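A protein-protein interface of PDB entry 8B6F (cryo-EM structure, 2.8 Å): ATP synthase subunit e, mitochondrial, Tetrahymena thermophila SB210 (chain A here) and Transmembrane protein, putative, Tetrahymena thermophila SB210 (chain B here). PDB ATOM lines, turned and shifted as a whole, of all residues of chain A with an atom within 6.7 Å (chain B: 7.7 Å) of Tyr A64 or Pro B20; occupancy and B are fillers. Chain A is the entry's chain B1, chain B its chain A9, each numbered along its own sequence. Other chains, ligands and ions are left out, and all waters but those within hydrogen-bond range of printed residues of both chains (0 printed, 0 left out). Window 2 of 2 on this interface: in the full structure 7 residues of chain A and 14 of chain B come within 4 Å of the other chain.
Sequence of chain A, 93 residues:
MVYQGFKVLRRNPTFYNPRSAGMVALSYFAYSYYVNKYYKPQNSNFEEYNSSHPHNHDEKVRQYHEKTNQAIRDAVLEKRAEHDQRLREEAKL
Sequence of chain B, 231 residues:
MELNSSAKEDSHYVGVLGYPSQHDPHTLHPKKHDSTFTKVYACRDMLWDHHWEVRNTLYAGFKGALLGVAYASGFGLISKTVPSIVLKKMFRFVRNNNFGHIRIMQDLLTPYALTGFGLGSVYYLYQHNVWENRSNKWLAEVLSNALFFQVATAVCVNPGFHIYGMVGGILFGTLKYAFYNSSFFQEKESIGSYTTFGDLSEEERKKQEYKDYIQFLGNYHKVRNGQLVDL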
ATOM      1  N   HIS A  57      18.916 -21.283  -4.499  1.00  0.00           N
ATOM      2  CA  HIS A  57      18.192 -22.276  -3.712  1.00  0.00           C
ATOM      3  C   HIS A  57      17.324 -21.613  -2.650  1.00  0.00           C
ATOM      4  O   HIS A  57      16.183 -22.029  -2.421  1.00  0.00           O
ATOM      5  CB  HIS A  57      19.174 -23.252  -3.065  1.00  0.00           C
ATOM      6  CG  HIS A  57      18.512 -24.366  -2.315  1.00  0.00           C
ATOM      7  ND1 HIS A  57      17.598 -25.219  -2.898  1.00  0.00           N
ATOM      8  CD2 HIS A  57      18.633 -24.770  -1.029  1.00  0.00           C
ATOM      9  CE1 HIS A  57      17.184 -26.097  -2.002  1.00  0.00           C
ATOM     10  NE2 HIS A  57      17.798 -25.847  -0.861  1.00  0.00           N
ATOM     11  N   GLU A  59      15.910 -18.620  -2.707  1.00  0.00           N
ATOM     12  CA  GLU A  59      14.728 -18.032  -3.327  1.00  0.00           C
ATOM     13  C   GLU A  59      13.734 -19.105  -3.749  1.00  0.00           C
ATOM     14  O   GLU A  59      12.521 -18.928  -3.590  1.00  0.00           O
ATOM     15  CB  GLU A  59      15.136 -17.178  -4.526  1.00  0.00           C
ATOM     16  CG  GLU A  59      13.964 -16.553  -5.270  1.00  0.00           C
ATOM     17  CD  GLU A  59      13.098 -15.680  -4.384  1.00  0.00           C
ATOM     18  OE1 GLU A  59      13.576 -15.258  -3.311  1.00  0.00           O
ATOM     19  OE2 GLU A  59      11.938 -15.417  -4.759  1.00  0.00           O
ATOM     20  N   LYS A  60      14.221 -20.222  -4.292  1.00  0.00           N
ATOM     21  CA  LYS A  60      13.318 -21.309  -4.654  1.00  0.00           C
ATOM     22  C   LYS A  60      12.580 -21.833  -3.430  1.00  0.00           C
ATOM     23  O   LYS A  60      11.373 -22.093  -3.487  1.00  0.00           O
ATOM     24  CB  LYS A  60      14.091 -22.438  -5.335  1.00  0.00           C
ATOM     25  CG  LYS A  60      14.614 -22.081  -6.713  1.00  0.00           C
ATOM     26  CD  LYS A  60      15.079 -23.313  -7.475  1.00  0.00           C
ATOM     27  CE  LYS A  60      16.232 -24.010  -6.770  1.00  0.00           C
ATOM     28  NZ  LYS A  60      16.736 -25.174  -7.551  1.00  0.00           N
ATOM     29  N   VAL A  61      13.291 -22.000  -2.315  1.00  0.00           N
ATOM     30  CA  VAL A  61      12.652 -22.472  -1.090  1.00  0.00           C
ATOM     31  C   VAL A  61      11.614 -21.467  -0.608  1.00  0.00           C
ATOM     32  O   VAL A  61      10.515 -21.843  -0.184  1.00  0.00           O
ATOM     33  CB  VAL A  61      13.713 -22.754  -0.011  1.00  0.00           C
ATOM     34  CG1 VAL A  61      13.058 -23.032   1.337  1.00  0.00           C
ATOM     35  CG2 VAL A  61      14.581 -23.928  -0.424  1.00  0.00           C
ATOM     36  N   ARG A  62      11.939 -20.173  -0.671  1.00  0.00           N
ATOM     37  CA  ARG A  62      10.988 -19.155  -0.237  1.00  0.00           C
ATOM     38  C   ARG A  62       9.725 -19.190  -1.083  1.00  0.00           C
ATOM     39  O   ARG A  62       8.611 -19.117  -0.552  1.00  0.00           O
ATOM     40  CB  ARG A  62      11.636 -17.773  -0.300  1.00  0.00           C
ATOM     41  CG  ARG A  62      10.814 -16.682   0.368  1.00  0.00           C
ATOM     42  CD  ARG A  62      11.340 -15.299   0.029  1.00  0.00           C
ATOM     43  NE  ARG A  62      11.224 -15.018  -1.397  1.00  0.00           N
ATOM     44  CZ  ARG A  62      10.100 -14.661  -2.002  1.00  0.00           C
ATOM     45  NH1 ARG A  62       8.964 -14.538  -1.334  1.00  0.00           N
ATOM     46  NH2 ARG A  62      10.113 -14.427  -3.310  1.00  0.00           N
ATOM     47  N   GLN A  63       9.874 -19.301  -2.401  1.00  0.00           N
ATOM     48  CA  GLN A  63       8.704 -19.364  -3.269  1.00  0.00           C
ATOM     49  C   GLN A  63       7.903 -20.634  -3.015  1.00  0.00           C
ATOM     50  O   GLN A  63       6.670 -20.618  -3.068  1.00  0.00           O
ATOM     51  CB  GLN A  63       9.133 -19.265  -4.732  1.00  0.00           C
ATOM     52  CG  GLN A  63       9.742 -17.917  -5.076  1.00  0.00           C
ATOM     53  CD  GLN A  63      10.097 -17.794  -6.537  1.00  0.00           C
ATOM     54  OE1 GLN A  63      10.030 -18.764  -7.290  1.00  0.00           O
ATOM     55  NE2 GLN A  63      10.471 -16.590  -6.953  1.00  0.00           N
ATOM     56  N   TYR A  64       8.588 -21.747  -2.740  1.00  0.00           N
ATOM     57  CA  TYR A  64       7.883 -22.973  -2.383  1.00  0.00           C
ATOM     58  C   TYR A  64       7.068 -22.779  -1.111  1.00  0.00           C
ATOM     59  O   TYR A  64       5.911 -23.209  -1.033  1.00  0.00           O
ATOM     60  CB  TYR A  64       8.872 -24.124  -2.215  1.00  0.00           C
ATOM     61  CG  TYR A  64       8.221 -25.404  -1.753  1.00  0.00           C
ATOM     62  CD1 TYR A  64       7.566 -26.233  -2.653  1.00  0.00           C
ATOM     63  CD2 TYR A  64       8.263 -25.788  -0.419  1.00  0.00           C
ATOM     64  CE1 TYR A  64       6.969 -27.405  -2.239  1.00  0.00           C
ATOM     65  CE2 TYR A  64       7.669 -26.958   0.004  1.00  0.00           C
ATOM     66  CZ  TYR A  64       7.025 -27.762  -0.912  1.00  0.00           C
ATOM     67  OH  TYR A  64       6.432 -28.928  -0.497  1.00  0.00           O
ATOM     68  N   HIS A  65       7.657 -22.141  -0.099  1.00  0.00           N
ATOM     69  CA  HIS A  65       6.921 -21.858   1.129  1.00  0.00           C
ATOM     70  C   HIS A  65       5.688 -21.016   0.834  1.00  0.00           C
ATOM     71  O   HIS A  65       4.596 -21.291   1.341  1.00  0.00           O
ATOM     72  CB  HIS A  65       7.825 -21.142   2.133  1.00  0.00           C
ATOM     73  CG  HIS A  65       8.707 -22.059   2.921  1.00  0.00           C
ATOM     74  ND1 HIS A  65       8.587 -22.212   4.285  1.00  0.00           N
ATOM     75  CD2 HIS A  65       9.729 -22.861   2.542  1.00  0.00           C
ATOM     76  CE1 HIS A  65       9.493 -23.072   4.712  1.00  0.00           C
ATOM     77  NE2 HIS A  65      10.200 -23.481   3.674  1.00  0.00           N
ATOM     78  N   GLU A  66       5.847 -19.976   0.015  1.00  0.00           N
ATOM     79  CA  GLU A  66       4.728 -19.095  -0.296  1.00  0.00           C
ATOM     80  C   GLU A  66       3.596 -19.860  -0.972  1.00  0.00           C
ATOM     81  O   GLU A  66       2.435 -19.763  -0.560  1.00  0.00           O
ATOM     82  CB  GLU A  66       5.207 -17.947  -1.184  1.00  0.00           C
ATOM     83  CG  GLU A  66       4.120 -16.954  -1.558  1.00  0.00           C
ATOM     84  CD  GLU A  66       4.626 -15.857  -2.475  1.00  0.00           C
ATOM     85  OE1 GLU A  66       5.783 -15.954  -2.936  1.00  0.00           O
ATOM     86  OE2 GLU A  66       3.870 -14.899  -2.735  1.00  0.00           O
ATOM     87  N   LYS A  67       3.913 -20.622  -2.019  1.00  0.00           N
ATOM     88  CA  LYS A  67       2.870 -21.340  -2.745  1.00  0.00           C
ATOM     89  C   LYS A  67       2.216 -22.400  -1.870  1.00  0.00           C
ATOM     90  O   LYS A  67       1.000 -22.604  -1.939  1.00  0.00           O
ATOM     91  CB  LYS A  67       3.443 -21.968  -4.015  1.00  0.00           C
ATOM     92  CG  LYS A  67       4.496 -23.028  -3.763  1.00  0.00           C
ATOM     93  CD  LYS A  67       5.084 -23.562  -5.063  1.00  0.00           C
ATOM     94  CE  LYS A  67       4.056 -24.327  -5.886  1.00  0.00           C
ATOM     95  NZ  LYS A  67       3.459 -25.466  -5.135  1.00  0.00           N
ATOM     96  N   THR A  68       3.006 -23.092  -1.045  1.00  0.00           N
ATOM     97  CA  THR A  68       2.438 -24.114  -0.174  1.00  0.00           C
ATOM     98  C   THR A  68       1.486 -23.502   0.845  1.00  0.00           C
ATOM     99  O   THR A  68       0.402 -24.043   1.094  1.00  0.00           O
ATOM    100  CB  THR A  68       3.557 -24.878   0.534  1.00  0.00           C
ATOM    101  OG1 THR A  68       4.409 -25.493  -0.440  1.00  0.00           O
ATOM    102  CG2 THR A  68       2.983 -25.953   1.446  1.00  0.00           C
ATOM    103  N   ASN A  69       1.868 -22.373   1.443  1.00  0.00           N
ATOM    104  CA  ASN A  69       0.976 -21.711   2.389  1.00  0.00           C
ATOM    105  C   ASN A  69      -0.298 -21.244   1.700  1.00  0.00           C
ATOM    106  O   ASN A  69      -1.394 -21.365   2.258  1.00  0.00           O
ATOM    107  CB  ASN A  69       1.691 -20.534   3.050  1.00  0.00           C
ATOM    108  CG  ASN A  69       2.855 -20.970   3.912  1.00  0.00           C
ATOM    109  OD1 ASN A  69       2.797 -22.005   4.576  1.00  0.00           O
ATOM    110  ND2 ASN A  69       3.923 -20.185   3.903  1.00  0.00           N
ATOM    111  N   GLU B   9      20.014 -35.726   1.992  1.00  0.00           N
ATOM    112  CA  GLU B   9      18.745 -35.288   1.434  1.00  0.00           C
ATOM    113  C   GLU B   9      17.995 -36.496   0.898  1.00  0.00           C
ATOM    114  O   GLU B   9      18.587 -37.373   0.263  1.00  0.00           O
ATOM    115  CB  GLU B   9      18.953 -34.266   0.311  1.00  0.00           C
ATOM    116  CG  GLU B   9      17.663 -33.827  -0.375  1.00  0.00           C
ATOM    117  CD  GLU B   9      17.918 -32.997  -1.616  1.00  0.00           C
ATOM    118  OE1 GLU B   9      19.078 -32.587  -1.826  1.00  0.00           O
ATOM    119  OE2 GLU B   9      16.964 -32.760  -2.384  1.00  0.00           O
ATOM    120  N   TYR B  13      11.553 -38.158  -1.252  1.00  0.00           N
ATOM    121  CA  TYR B  13      10.587 -37.406  -0.457  1.00  0.00           C
ATOM    122  C   TYR B  13      10.433 -35.979  -0.971  1.00  0.00           C
ATOM    123  O   TYR B  13       9.312 -35.467  -1.065  1.00  0.00           O
ATOM    124  CB  TYR B  13      11.006 -37.412   1.010  1.00  0.00           C
ATOM    125  CG  TYR B  13       9.871 -37.115   1.956  1.00  0.00           C
ATOM    126  CD1 TYR B  13       8.824 -38.015   2.103  1.00  0.00           C
ATOM    127  CD2 TYR B  13       9.852 -35.955   2.716  1.00  0.00           C
ATOM    128  CE1 TYR B  13       7.786 -37.767   2.965  1.00  0.00           C
ATOM    129  CE2 TYR B  13       8.812 -35.697   3.587  1.00  0.00           C
ATOM    130  CZ  TYR B  13       7.782 -36.611   3.705  1.00  0.00           C
ATOM    131  OH  TYR B  13       6.736 -36.381   4.563  1.00  0.00           O
ATOM    132  N   VAL B  14      11.542 -35.312  -1.289  1.00  0.00           N
ATOM    133  CA  VAL B  14      11.453 -33.949  -1.801  1.00  0.00           C
ATOM    134  C   VAL B  14      10.752 -33.938  -3.154  1.00  0.00           C
ATOM    135  O   VAL B  14      10.002 -33.008  -3.472  1.00  0.00           O
ATOM    136  CB  VAL B  14      12.849 -33.301  -1.881  1.00  0.00           C
ATOM    137  CG1 VAL B  14      13.493 -33.252  -0.507  1.00  0.00           C
ATOM    138  CG2 VAL B  14      13.736 -34.038  -2.864  1.00  0.00           C
ATOM    139  N   GLY B  15      10.982 -34.967  -3.970  1.00  0.00           N
ATOM    140  CA  GLY B  15      10.318 -35.033  -5.261  1.00  0.00           C
ATOM    141  C   GLY B  15       8.817 -35.220  -5.147  1.00  0.00           C
ATOM    142  O   GLY B  15       8.049 -34.570  -5.859  1.00  0.00           O
ATOM    143  N   VAL B  16       8.375 -36.108  -4.255  1.00  0.00           N
ATOM    144  CA  VAL B  16       6.940 -36.321  -4.096  1.00  0.00           C
ATOM    145  C   VAL B  16       6.280 -35.080  -3.508  1.00  0.00           C
ATOM    146  O   VAL B  16       5.147 -34.737  -3.863  1.00  0.00           O
ATOM    147  CB  VAL B  16       6.667 -37.569  -3.237  1.00  0.00           C
ATOM    148  CG1 VAL B  16       7.203 -38.813  -3.921  1.00  0.00           C
ATOM    149  CG2 VAL B  16       7.280 -37.418  -1.861  1.00  0.00           C
ATOM    150  N   LEU B  17       6.968 -34.390  -2.596  1.00  0.00           N
ATOM    151  CA  LEU B  17       6.416 -33.174  -2.016  1.00  0.00           C
ATOM    152  C   LEU B  17       6.473 -31.984  -2.965  1.00  0.00           C
ATOM    153  O   LEU B  17       5.715 -31.028  -2.777  1.00  0.00           O
ATOM    154  CB  LEU B  17       7.157 -32.808  -0.727  1.00  0.00           C
ATOM    155  CG  LEU B  17       6.965 -33.702   0.499  1.00  0.00           C
ATOM    156  CD1 LEU B  17       7.755 -33.138   1.664  1.00  0.00           C
ATOM    157  CD2 LEU B  17       5.501 -33.861   0.872  1.00  0.00           C
ATOM    158  N   GLY B  18       7.338 -32.020  -3.974  1.00  0.00           N
ATOM    159  CA  GLY B  18       7.579 -30.853  -4.793  1.00  0.00           C
ATOM    160  C   GLY B  18       8.595 -29.889  -4.225  1.00  0.00           C
ATOM    161  O   GLY B  18       8.833 -28.837  -4.830  1.00  0.00           O
ATOM    162  N   TYR B  19       9.198 -30.214  -3.089  1.00  0.00           N
ATOM    163  CA  TYR B  19      10.191 -29.338  -2.488  1.00  0.00           C
ATOM    164  C   TYR B  19      11.389 -29.200  -3.426  1.00  0.00           C
ATOM    165  O   TYR B  19      11.809 -30.185  -4.042  1.00  0.00           O
ATOM    166  CB  TYR B  19      10.635 -29.913  -1.141  1.00  0.00           C
ATOM    167  CG  TYR B  19      11.443 -28.976  -0.275  1.00  0.00           C
ATOM    168  CD1 TYR B  19      10.821 -28.103   0.605  1.00  0.00           C
ATOM    169  CD2 TYR B  19      12.829 -28.983  -0.320  1.00  0.00           C
ATOM    170  CE1 TYR B  19      11.555 -27.252   1.404  1.00  0.00           C
ATOM    171  CE2 TYR B  19      13.574 -28.136   0.476  1.00  0.00           C
ATOM    172  CZ  TYR B  19      12.930 -27.273   1.337  1.00  0.00           C
ATOM    173  OH  TYR B  19      13.665 -26.428   2.133  1.00  0.00           O
ATOM    174  N   PRO B  20      11.956 -28.001  -3.572  1.00  0.00           N
ATOM    175  CA  PRO B  20      13.138 -27.861  -4.431  1.00  0.00           C
ATOM    176  C   PRO B  20      14.274 -28.745  -3.938  1.00  0.00           C
ATOM    177  O   PRO B  20      14.508 -28.877  -2.737  1.00  0.00           O
ATOM    178  CB  PRO B  20      13.486 -26.373  -4.323  1.00  0.00           C
ATOM    179  CG  PRO B  20      12.832 -25.911  -3.071  1.00  0.00           C
ATOM    180  CD  PRO B  20      11.586 -26.724  -2.941  1.00  0.00           C
ATOM    181  N   SER B  21      14.988 -29.343  -4.886  1.00  0.00           N
ATOM    182  CA  SER B  21      16.031 -30.312  -4.585  1.00  0.00           C
ATOM    183  C   SER B  21      17.400 -29.663  -4.726  1.00  0.00           C
ATOM    184  O   SER B  21      17.672 -28.985  -5.722  1.00  0.00           O
ATOM    185  CB  SER B  21      15.923 -31.522  -5.514  1.00  0.00           C
ATOM    186  OG  SER B  21      16.923 -32.480  -5.221  1.00  0.00           O
ATOM    187  N   GLN B  22      18.256 -29.872  -3.725  1.00  0.00           N
ATOM    188  CA  GLN B  22      19.616 -29.350  -3.765  1.00  0.00           C
ATOM    189  C   GLN B  22      20.486 -30.048  -4.802  1.00  0.00           C
ATOM    190  O   GLN B  22      21.580 -29.555  -5.099  1.00  0.00           O
ATOM    191  CB  GLN B  22      20.258 -29.476  -2.382  1.00  0.00           C
ATOM    192  CG  GLN B  22      19.607 -28.593  -1.331  1.00  0.00           C
ATOM    193  CD  GLN B  22      20.069 -28.919   0.073  1.00  0.00           C
ATOM    194  OE1 GLN B  22      20.162 -30.084   0.453  1.00  0.00           O
ATOM    195  NE2 GLN B  22      20.366 -27.886   0.852  1.00  0.00           N
ATOM    196  N   HIS B  23      20.033 -31.168  -5.356  1.00  0.00           N
ATOM    197  CA  HIS B  23      20.782 -31.901  -6.367  1.00  0.00           C
ATOM    198  C   HIS B  23      20.543 -31.374  -7.774  1.00  0.00           C
ATOM    199  O   HIS B  23      21.072 -31.948  -8.731  1.00  0.00           O
ATOM    200  CB  HIS B  23      20.426 -33.389  -6.308  1.00  0.00           C
ATOM    201  CG  HIS B  23      20.855 -34.060  -5.041  1.00  0.00           C
ATOM    202  ND1 HIS B  23      21.773 -33.503  -4.176  1.00  0.00           N
ATOM    203  CD2 HIS B  23      20.488 -35.240  -4.488  1.00  0.00           C
ATOM    204  CE1 HIS B  23      21.953 -34.311  -3.148  1.00  0.00           C
ATOM    205  NE2 HIS B  23      21.186 -35.374  -3.312  1.00  0.00           N
ATOM    206  N   ASP B  24      19.767 -30.304  -7.925  1.00  0.00           N
ATOM    207  CA  ASP B  24      19.558 -29.731  -9.242  1.00  0.00           C
ATOM    208  C   ASP B  24      20.895 -29.272  -9.821  1.00  0.00           C
ATOM    209  O   ASP B  24      21.805 -28.892  -9.078  1.00  0.00           O
ATOM    210  CB  ASP B  24      18.586 -28.556  -9.167  1.00  0.00           C
ATOM    211  CG  ASP B  24      17.155 -29.000  -8.950  1.00  0.00           C
ATOM    212  OD1 ASP B  24      16.919 -30.222  -8.849  1.00  0.00           O
ATOM    213  OD2 ASP B  24      16.263 -28.127  -8.884  1.00  0.00           O
ATOM    214  N   LYS B 188      14.355 -33.038   8.325  1.00  0.00           N
ATOM    215  CA  LYS B 188      13.519 -32.448   7.286  1.00  0.00           C
ATOM    216  C   LYS B 188      12.355 -33.360   6.921  1.00  0.00           C
ATOM    217  O   LYS B 188      11.719 -33.168   5.880  1.00  0.00           O
ATOM    218  CB  LYS B 188      14.353 -32.119   6.047  1.00  0.00           C
ATOM    219  CG  LYS B 188      15.366 -31.009   6.273  1.00  0.00           C
ATOM    220  CD  LYS B 188      16.036 -30.592   4.974  1.00  0.00           C
ATOM    221  CE  LYS B 188      16.965 -29.407   5.192  1.00  0.00           C
ATOM    222  NZ  LYS B 188      17.628 -28.977   3.929  1.00  0.00           N
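Among the printed residues, merely in contact across the chains: His A57 with Gln B22 (3.3 Å), Tyr A64 with Tyr B19 (3.4 Å), Tyr A64 with Gly B18 (3.5 Å), Val A61 with Tyr B19 (3.5 Å), Val A61 with Pro B20 (3.7 Å), Tyr A64 with Pro B20 (3.8 Å) and His A57 with Pro B20 (3.9 Å).
Of the 12 printed residues of chain A, 4 touch a printed residue of chain B. Hydrophobic or aromatic side chains of chain A that line the printed part of chain B: His A57, Val A61 and Tyr A64. Among the printed residues, 9 pairs touch across the chains. Among the printed residues, Asp or Glu carboxylates within 4 Å of a Lys or Arg side-chain nitrogen of the other chain: Lys A60 with Asp B24 (3.3 Å).
The side-chain hydroxyl (OH) of Tyr A64 lies within hydrogen-bond range of the backbone carbonyl oxygen (O) of Leu B17, 3.2 Å away. The side-chain carboxylate of Asp B24 lies within salt-bridge range of the side-chain amino group of Lys A60.
Of the printed residues of chain B, Val A61 touches Tyr B19 and Pro B20. Of chain B, only Leu B17, Gly B18, Tyr B19 and Pro B20 come within 4 Å of Tyr A64. Printed residues of chain A within 4 Å of Leu B17: Tyr A64. Of the printed residues of chain A, Tyr B19 touches Val A61 (3.5 Å) and Tyr A64 (3.4 Å). Pro B20 touches just these residues of chain A: His A57, Val A61 and Tyr A64. Printed residues of chain A within 4 Å of Gln B22: His A57 (3.3 Å). Printed residues of chain A within 4 Å of Asp B24: Lys A60 (3.3 Å). The nearest residue of chain B that does not touch Tyr A64 is Val B14 (6.2 Å). The nearest printed residue of chain A that does not touch Tyr B19 is His A65 (4.6 Å).
The side-chain carboxylate of Glu B9 sits close to the backbone NH of Gln B22, 3.4 Å away. The backbone carbonyl oxygen of Val B14 is in hydrogen-bond range of the backbone NH of Tyr B19, 2.9 Å away. OG1 of Thr A68 lies within hydrogen-bond range of O of Tyr A64 (2.8 Å).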
